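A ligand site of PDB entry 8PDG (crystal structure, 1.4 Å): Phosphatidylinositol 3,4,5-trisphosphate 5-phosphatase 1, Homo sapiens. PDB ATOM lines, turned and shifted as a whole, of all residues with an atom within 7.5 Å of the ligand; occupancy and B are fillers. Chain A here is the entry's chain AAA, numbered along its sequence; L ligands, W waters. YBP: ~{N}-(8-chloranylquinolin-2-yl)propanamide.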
ATOM      1  N   SER A 109      30.847  17.943 -17.605  1.00  0.00           N
ATOM      2  CA  SER A 109      31.389  18.414 -16.320  1.00  0.00           C
ATOM      3  C   SER A 109      31.419  17.275 -15.311  1.00  0.00           C
ATOM      4  O   SER A 109      30.932  16.146 -15.624  1.00  0.00           O
ATOM      5  CB  SER A 109      30.513  19.587 -15.871  1.00  0.00           C
ATOM      6  OG  SER A 109      29.210  19.114 -15.582  1.00  0.00           O
ATOM      7  N   HIS A 110      31.946  17.532 -14.123  1.00  0.00           N
ATOM      8  CA  HIS A 110      31.963  16.530 -13.036  1.00  0.00           C
ATOM      9  C   HIS A 110      32.587  15.215 -13.481  1.00  0.00           C
ATOM     10  O   HIS A 110      32.044  14.150 -13.185  1.00  0.00           O
ATOM     11  CB  HIS A 110      30.539  16.323 -12.520  1.00  0.00           C
ATOM     12  CG  HIS A 110      30.057  17.485 -11.739  1.00  0.00           C
ATOM     13  ND1 HIS A 110      29.104  18.329 -12.224  1.00  0.00           N
ATOM     14  CD2 HIS A 110      30.418  17.947 -10.540  1.00  0.00           C
ATOM     15  CE1 HIS A 110      28.864  19.271 -11.358  1.00  0.00           C
ATOM     16  NE2 HIS A 110      29.659  19.058 -10.303  1.00  0.00           N
ATOM     17  N   ILE A 111      33.727  15.281 -14.149  1.00  0.00           N
ATOM     18  CA  ILE A 111      34.452  14.091 -14.608  1.00  0.00           C
ATOM     19  C   ILE A 111      35.122  13.423 -13.414  1.00  0.00           C
ATOM     20  O   ILE A 111      35.851  14.069 -12.656  1.00  0.00           O
ATOM     21  CB  ILE A 111      35.457  14.445 -15.711  1.00  0.00           C
ATOM     22  CG1 ILE A 111      34.763  15.071 -16.921  1.00  0.00           C
ATOM     23  CG2 ILE A 111      36.201  13.216 -16.157  1.00  0.00           C
ATOM     24  CD1 ILE A 111      35.727  15.867 -17.780  1.00  0.00           C
ATOM     25  N   CYS A 112      34.827  12.147 -13.247  1.00  0.00           N
ATOM     26  CA  CYS A 112      35.436  11.303 -12.175  1.00  0.00           C
ATOM     27  C   CYS A 112      35.946  10.003 -12.772  1.00  0.00           C
ATOM     28  O   CYS A 112      35.382   9.494 -13.749  1.00  0.00           O
ATOM     29  CB  CYS A 112      34.477  10.971 -11.055  1.00  0.00           C
ATOM     30  SG  CYS A 112      34.091  12.415 -10.041  1.00  0.00           S
ATOM     31  N   THR A 113      37.029   9.500 -12.188  1.00  0.00           N
ATOM     32  CA  THR A 113      37.608   8.187 -12.517  1.00  0.00           C
ATOM     33  C   THR A 113      37.826   7.446 -11.220  1.00  0.00           C
ATOM     34  O   THR A 113      38.004   8.057 -10.154  1.00  0.00           O
ATOM     35  CB  THR A 113      38.921   8.302 -13.311  1.00  0.00           C
ATOM     36  OG1 THR A 113      39.904   8.961 -12.514  1.00  0.00           O
ATOM     37  CG2 THR A 113      38.781   9.084 -14.592  1.00  0.00           C
ATOM     38  N   ASP A 114      37.787   6.125 -11.299  1.00  0.00           N
ATOM     39  CA  ASP A 114      38.118   5.278 -10.140  1.00  0.00           C
ATOM     40  C   ASP A 114      38.437   3.866 -10.607  1.00  0.00           C
ATOM     41  O   ASP A 114      38.207   3.517 -11.802  1.00  0.00           O
ATOM     42  CB  ASP A 114      36.974   5.256  -9.130  1.00  0.00           C
ATOM     43  CG  ASP A 114      37.375   4.794  -7.745  1.00  0.00           C
ATOM     44  OD1 ASP A 114      38.601   4.877  -7.427  1.00  0.00           O
ATOM     45  OD2 ASP A 114      36.513   4.279  -7.020  1.00  0.00           O
ATOM     46  N   SER A 133      32.872   8.558 -14.860  1.00  0.00           N
ATOM     47  CA  SER A 133      31.552   9.202 -14.919  1.00  0.00           C
ATOM     48  C   SER A 133      31.661  10.670 -15.180  1.00  0.00           C
ATOM     49  O   SER A 133      32.723  11.262 -14.989  1.00  0.00           O
ATOM     50  CB  SER A 133      30.792   8.963 -13.644  1.00  0.00           C
ATOM     51  OG  SER A 133      31.439   9.526 -12.526  1.00  0.00           O
ATOM     52  N   PHE A 134      30.590  11.234 -15.705  1.00  0.00           N
ATOM     53  CA  PHE A 134      30.488  12.682 -15.900  1.00  0.00           C
ATOM     54  C   PHE A 134      29.030  13.015 -16.194  1.00  0.00           C
ATOM     55  O   PHE A 134      28.161  12.154 -16.471  1.00  0.00           O
ATOM     56  CB  PHE A 134      31.420  13.147 -17.031  1.00  0.00           C
ATOM     57  CG  PHE A 134      31.290  12.441 -18.358  1.00  0.00           C
ATOM     58  CD1 PHE A 134      32.025  11.302 -18.631  1.00  0.00           C
ATOM     59  CD2 PHE A 134      30.414  12.881 -19.329  1.00  0.00           C
ATOM     60  CE1 PHE A 134      31.927  10.652 -19.832  1.00  0.00           C
ATOM     61  CE2 PHE A 134      30.340  12.257 -20.567  1.00  0.00           C
ATOM     62  CZ  PHE A 134      31.094  11.124 -20.814  1.00  0.00           C
ATOM     63  N   MET A 135      28.778  14.298 -16.149  1.00  0.00           N
ATOM     64  CA  MET A 135      27.501  14.879 -16.581  1.00  0.00           C
ATOM     65  C   MET A 135      27.633  15.371 -18.033  1.00  0.00           C
ATOM     66  O   MET A 135      28.669  15.994 -18.382  1.00  0.00           O
ATOM     67  CB  MET A 135      27.145  16.013 -15.597  1.00  0.00           C
ATOM     68  CG  MET A 135      25.682  16.262 -15.455  1.00  0.00           C
ATOM     69  SD  MET A 135      25.373  17.520 -14.205  1.00  0.00           S
ATOM     70  CE  MET A 135      23.587  17.427 -14.128  1.00  0.00           C
ATOM     71  N   PHE A 136      26.615  15.133 -18.833  1.00  0.00           N
ATOM     72  CA  PHE A 136      26.500  15.626 -20.213  1.00  0.00           C
ATOM     73  C   PHE A 136      25.240  16.474 -20.176  1.00  0.00           C
ATOM     74  O   PHE A 136      24.133  15.911 -20.047  1.00  0.00           O
ATOM     75  CB  PHE A 136      26.388  14.511 -21.245  1.00  0.00           C
ATOM     76  CG  PHE A 136      26.308  14.995 -22.672  1.00  0.00           C
ATOM     77  CD1 PHE A 136      25.116  15.455 -23.235  1.00  0.00           C
ATOM     78  CD2 PHE A 136      27.463  15.056 -23.453  1.00  0.00           C
ATOM     79  CE1 PHE A 136      25.102  15.960 -24.520  1.00  0.00           C
ATOM     80  CE2 PHE A 136      27.422  15.518 -24.740  1.00  0.00           C
ATOM     81  CZ  PHE A 136      26.234  15.997 -25.278  1.00  0.00           C
ATOM     82  N   ASN A 137      25.390  17.782 -20.138  1.00  0.00           N
ATOM     83  CA  ASN A 137      24.256  18.707 -19.857  1.00  0.00           C
ATOM     84  C   ASN A 137      23.466  18.196 -18.631  1.00  0.00           C
ATOM     85  O   ASN A 137      24.077  18.081 -17.536  1.00  0.00           O
ATOM     86  CB  ASN A 137      23.397  18.855 -21.116  1.00  0.00           C
ATOM     87  CG  ASN A 137      24.069  19.768 -22.129  1.00  0.00           C
ATOM     88  OD1 ASN A 137      24.927  20.576 -21.794  1.00  0.00           O
ATOM     89  ND2 ASN A 137      23.630  19.648 -23.367  1.00  0.00           N
ATOM     90  N   GLY A 138      22.194  17.836 -18.756  1.00  0.00           N
ATOM     91  CA  GLY A 138      21.417  17.411 -17.569  1.00  0.00           C
ATOM     92  C   GLY A 138      21.454  15.926 -17.302  1.00  0.00           C
ATOM     93  O   GLY A 138      20.670  15.473 -16.450  1.00  0.00           O
ATOM     94  N   THR A 139      22.315  15.167 -18.003  1.00  0.00           N
ATOM     95  CA  THR A 139      22.259  13.698 -18.007  1.00  0.00           C
ATOM     96  C   THR A 139      23.548  13.139 -17.397  1.00  0.00           C
ATOM     97  O   THR A 139      24.618  13.622 -17.735  1.00  0.00           O
ATOM     98  CB  THR A 139      22.030  13.160 -19.418  1.00  0.00           C
ATOM     99  OG1 THR A 139      20.795  13.709 -19.913  1.00  0.00           O
ATOM    100  CG2 THR A 139      21.992  11.666 -19.430  1.00  0.00           C
ATOM    101  N   SER A 140      23.407  12.238 -16.453  1.00  0.00           N
ATOM    102  CA  SER A 140      24.564  11.612 -15.798  1.00  0.00           C
ATOM    103  C   SER A 140      24.893  10.273 -16.478  1.00  0.00           C
ATOM    104  O   SER A 140      23.982   9.514 -16.780  1.00  0.00           O
ATOM    105  CB  SER A 140      24.331  11.500 -14.335  1.00  0.00           C
ATOM    106  OG  SER A 140      23.254  10.617 -14.122  1.00  0.00           O
ATOM    107  N   LEU A 141      26.167  10.092 -16.793  1.00  0.00           N
ATOM    108  CA  LEU A 141      26.673   8.953 -17.597  1.00  0.00           C
ATOM    109  C   LEU A 141      27.741   8.240 -16.771  1.00  0.00           C
ATOM    110  O   LEU A 141      28.645   8.885 -16.260  1.00  0.00           O
ATOM    111  CB  LEU A 141      27.220   9.401 -18.939  1.00  0.00           C
ATOM    112  CG  LEU A 141      26.226  10.101 -19.863  1.00  0.00           C
ATOM    113  CD1 LEU A 141      26.975  10.598 -21.075  1.00  0.00           C
ATOM    114  CD2 LEU A 141      25.053   9.212 -20.247  1.00  0.00           C
ATOM    115  N   GLY A 142      27.651   6.932 -16.677  1.00  0.00           N
ATOM    116  CA  GLY A 142      28.710   6.109 -16.045  1.00  0.00           C
ATOM    117  C   GLY A 142      29.156   4.974 -16.958  1.00  0.00           C
ATOM    118  O   GLY A 142      28.330   4.398 -17.723  1.00  0.00           O
ATOM    119  N   ALA A 170      33.768   4.301  -6.803  1.00  0.00           N
ATOM    120  CA  ALA A 170      33.283   5.621  -6.336  1.00  0.00           C
ATOM    121  C   ALA A 170      33.146   6.561  -7.519  1.00  0.00           C
ATOM    122  O   ALA A 170      34.126   7.253  -7.905  1.00  0.00           O
ATOM    123  CB  ALA A 170      34.217   6.184  -5.246  1.00  0.00           C
ATOM    124  N   LEU A 171      32.042   6.455  -8.232  1.00  0.00           N
ATOM    125  CA  LEU A 171      31.763   7.330  -9.380  1.00  0.00           C
ATOM    126  C   LEU A 171      30.463   8.062  -9.080  1.00  0.00           C
ATOM    127  O   LEU A 171      29.688   7.559  -8.254  1.00  0.00           O
ATOM    128  CB  LEU A 171      31.625   6.471 -10.646  1.00  0.00           C
ATOM    129  CG  LEU A 171      32.861   5.734 -11.122  1.00  0.00           C
ATOM    130  CD1 LEU A 171      32.497   4.898 -12.327  1.00  0.00           C
ATOM    131  CD2 LEU A 171      34.020   6.654 -11.477  1.00  0.00           C
ATOM    132  N   GLY A 172      30.208   9.103  -9.854  1.00  0.00           N
ATOM    133  CA  GLY A 172      28.940   9.828  -9.759  1.00  0.00           C
ATOM    134  C   GLY A 172      28.891  10.675  -8.500  1.00  0.00           C
ATOM    135  O   GLY A 172      29.934  10.846  -7.797  1.00  0.00           O
ATOM    136  N   ASP A 173      27.693  11.232  -8.262  1.00  0.00           N
ATOM    137  CA  ASP A 173      27.484  12.292  -7.242  1.00  0.00           C
ATOM    138  C   ASP A 173      27.643  11.686  -5.845  1.00  0.00           C
ATOM    139  O   ASP A 173      26.799  10.861  -5.424  1.00  0.00           O
ATOM    140  CB  ASP A 173      26.143  12.947  -7.504  1.00  0.00           C
ATOM    141  CG  ASP A 173      25.789  14.052  -6.530  1.00  0.00           C
ATOM    142  OD1 ASP A 173      26.635  14.360  -5.654  1.00  0.00           O
ATOM    143  OD2 ASP A 173      24.664  14.581  -6.636  1.00  0.00           O
ATOM    144  N   LYS A 174      28.660  12.097  -5.112  1.00  0.00           N
ATOM    145  CA  LYS A 174      28.953  11.545  -3.754  1.00  0.00           C
ATOM    146  C   LYS A 174      27.789  11.913  -2.798  1.00  0.00           C
ATOM    147  O   LYS A 174      27.616  11.236  -1.740  1.00  0.00           O
ATOM    148  CB  LYS A 174      30.350  11.971  -3.293  1.00  0.00           C
ATOM    149  CG  LYS A 174      30.604  13.443  -3.121  1.00  0.00           C
ATOM    150  CD  LYS A 174      32.041  13.719  -2.670  1.00  0.00           C
ATOM    151  CE  LYS A 174      33.075  13.689  -3.775  1.00  0.00           C
ATOM    152  NZ  LYS A 174      32.889  14.794  -4.747  1.00  0.00           N
ATOM    153  N   LYS A 175      26.967  12.909  -3.116  1.00  0.00           N
ATOM    154  CA  LYS A 175      25.793  13.232  -2.252  1.00  0.00           C
ATOM    155  C   LYS A 175      24.747  12.116  -2.304  1.00  0.00           C
ATOM    156  O   LYS A 175      23.886  12.044  -1.378  1.00  0.00           O
ATOM    157  CB  LYS A 175      25.158  14.561  -2.649  1.00  0.00           C
ATOM    158  CG  LYS A 175      26.015  15.796  -2.346  1.00  0.00           C
ATOM    159  CD  LYS A 175      25.349  17.141  -2.652  1.00  0.00           C
ATOM    160  CE  LYS A 175      24.741  17.199  -4.034  1.00  0.00           C
ATOM    161  NZ  LYS A 175      24.074  18.481  -4.354  1.00  0.00           N
ATOM    162  N   LEU A 176      24.794  11.235  -3.336  1.00  0.00           N
ATOM    163  CA  LEU A 176      23.870  10.100  -3.443  1.00  0.00           C
ATOM    164  C   LEU A 176      24.355   8.963  -2.538  1.00  0.00           C
ATOM    165  O   LEU A 176      24.605   7.848  -2.975  1.00  0.00           O
ATOM    166  CB  LEU A 176      23.740   9.699  -4.910  1.00  0.00           C
ATOM    167  CG  LEU A 176      23.158  10.789  -5.822  1.00  0.00           C
ATOM    168  CD1 LEU A 176      23.128  10.304  -7.275  1.00  0.00           C
ATOM    169  CD2 LEU A 176      21.739  11.088  -5.372  1.00  0.00           C
ATOM    170  N   ARG A 184      23.258   5.535  -9.730  1.00  0.00           N
ATOM    171  CA  ARG A 184      23.727   6.934  -9.771  1.00  0.00           C
ATOM    172  C   ARG A 184      23.614   7.592 -11.155  1.00  0.00           C
ATOM    173  O   ARG A 184      23.879   8.811 -11.218  1.00  0.00           O
ATOM    174  CB  ARG A 184      25.148   7.080  -9.207  1.00  0.00           C
ATOM    175  CG  ARG A 184      25.240   6.896  -7.702  1.00  0.00           C
ATOM    176  CD  ARG A 184      26.639   7.208  -7.181  1.00  0.00           C
ATOM    177  NE  ARG A 184      26.647   7.077  -5.741  1.00  0.00           N
ATOM    178  CZ  ARG A 184      27.625   7.492  -4.957  1.00  0.00           C
ATOM    179  NH1 ARG A 184      28.741   7.984  -5.502  1.00  0.00           N
ATOM    180  NH2 ARG A 184      27.519   7.391  -3.653  1.00  0.00           N
ATOM    181  N   PHE A 185      23.343   6.850 -12.220  1.00  0.00           N
ATOM    182  CA  PHE A 185      23.462   7.378 -13.576  1.00  0.00           C
ATOM    183  C   PHE A 185      22.185   7.227 -14.370  1.00  0.00           C
ATOM    184  O   PHE A 185      21.522   6.225 -14.322  1.00  0.00           O
ATOM    185  CB  PHE A 185      24.587   6.697 -14.335  1.00  0.00           C
ATOM    186  CG  PHE A 185      25.864   6.773 -13.549  1.00  0.00           C
ATOM    187  CD1 PHE A 185      26.493   7.987 -13.392  1.00  0.00           C
ATOM    188  CD2 PHE A 185      26.374   5.659 -12.947  1.00  0.00           C
ATOM    189  CE1 PHE A 185      27.614   8.101 -12.582  1.00  0.00           C
ATOM    190  CE2 PHE A 185      27.489   5.768 -12.131  1.00  0.00           C
ATOM    191  CZ  PHE A 185      28.107   7.000 -11.966  1.00  0.00           C
ATOM    192  N   SER A 361      18.042  15.333  -8.527  1.00  0.00           N
ATOM    193  CA  SER A 361      18.502  16.618  -9.100  1.00  0.00           C
ATOM    194  C   SER A 361      17.365  17.640  -9.161  1.00  0.00           C
ATOM    195  O   SER A 361      17.675  18.834  -9.241  1.00  0.00           O
ATOM    196  CB  SER A 361      19.110  16.404 -10.491  1.00  0.00           C
ATOM    197  OG  SER A 361      20.077  15.418 -10.423  1.00  0.00           O
HETATM  198  C1  YBP L   1      33.237  11.640  -8.803  1.00  0.00           C
HETATM  199  C2  YBP L   1      32.931  12.427  -7.584  1.00  0.00           C
HETATM  200  C3  YBP L   1      31.652  13.234  -7.661  1.00  0.00           C
HETATM  201  N1  YBP L   1      31.180  13.477  -8.922  1.00  0.00           N
HETATM  202  C4  YBP L   1      29.973  14.126  -9.251  1.00  0.00           C
HETATM  203  C5  YBP L   1      29.520  15.231  -8.464  1.00  0.00           C
HETATM  204  C6  YBP L   1      28.332  15.767  -8.802  1.00  0.00           C
HETATM  205  C7  YBP L   1      27.597  15.215  -9.875  1.00  0.00           C
HETATM  206  C8  YBP L   1      26.361  15.756 -10.255  1.00  0.00           C
HETATM  207  C9  YBP L   1      25.680  15.248 -11.314  1.00  0.00           C
HETATM  208  C10 YBP L   1      26.192  14.165 -12.053  1.00  0.00           C
HETATM  209  C11 YBP L   1      27.381  13.601 -11.725  1.00  0.00           C
HETATM  210  C12 YBP L   1      28.137  14.147 -10.622  1.00  0.00           C
HETATM  211  N2  YBP L   1      29.330  13.603 -10.270  1.00  0.00           N
HETATM  212 CL1  YBP L   1      27.982  12.332 -12.745  1.00  0.00          CL
HETATM  213  O1  YBP L   1      31.088  13.610  -6.619  1.00  0.00           O
HETATM  214  O   HOH W   1      30.860  12.136 -12.040  1.00  0.00           O
HETATM  215  O   HOH W   2      34.226  10.203  -5.357  1.00  0.00           O
HETATM  216  O   HOH W   3      31.980   9.441  -6.373  1.00  0.00           O
HETATM  217  O   HOH W   4      32.988  16.141  -9.570  1.00  0.00           O
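SG of Cys 112 is bonded to C1 of the ligand.
An oxygen (O1) of the ligand lies within hydrogen-bond range of the backbone NH (N) of Lys 174 (3.2 Å).
The side-chain amino group (NZ) of Lys 174 sits at hydrogen-bond distance from an oxygen (O1) of the ligand.
A nitrogen (N1) of the ligand lies close to the backbone carbonyl oxygen (O) of Gly 172 (3.1 Å).
The backbone NH (N) of Cys 112 sits at hydrogen-bond distance from the backbone carbonyl oxygen (O) of Ser 133 (2.9 Å).
The backbone NH (N) of Gly 172 is in hydrogen-bond range of the side-chain hydroxyl (OG) of Ser 133 (3.0 Å).
A ring nitrogen (ND1) of His 110 is in hydrogen-bond range of the side-chain hydroxyl (OG) of Ser 109 (3.5 Å).
The backbone NH (N) of Lys 175 sits at hydrogen-bond distance from the side-chain carboxylate (OD1) of Asp 173 (2.9 Å).
O of Asp 173 lies within hydrogen-bond range of NH1 of Arg 184, 3.5 Å away.
N of Leu 141 sits at hydrogen-bond distance from O of Phe 134 (2.9 Å).
N of Met 135 lies within hydrogen-bond range of O of Ser 109 (2.9 Å).
The side-chain hydroxyl (OG) of Ser 140 is in hydrogen-bond range of the backbone carbonyl oxygen (O) of Arg 184.
Merely in contact with the ligand: His 110, Asp 173, Phe 134, Met 135 and Ser 140.
Eight residues have an atom within 4 Å of the ligand: His 110, Cys 112, Phe 134, Met 135, Ser 140, Gly 172, Asp 173 and Lys 174.
Water W1 lies within hydrogen-bond range of the backbone carbonyl oxygen (O) of His 110 (2.6 Å), the side-chain hydroxyl (OG) of Ser 133 (2.7 Å) and a nitrogen (N2) of the ligand (2.8 Å).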
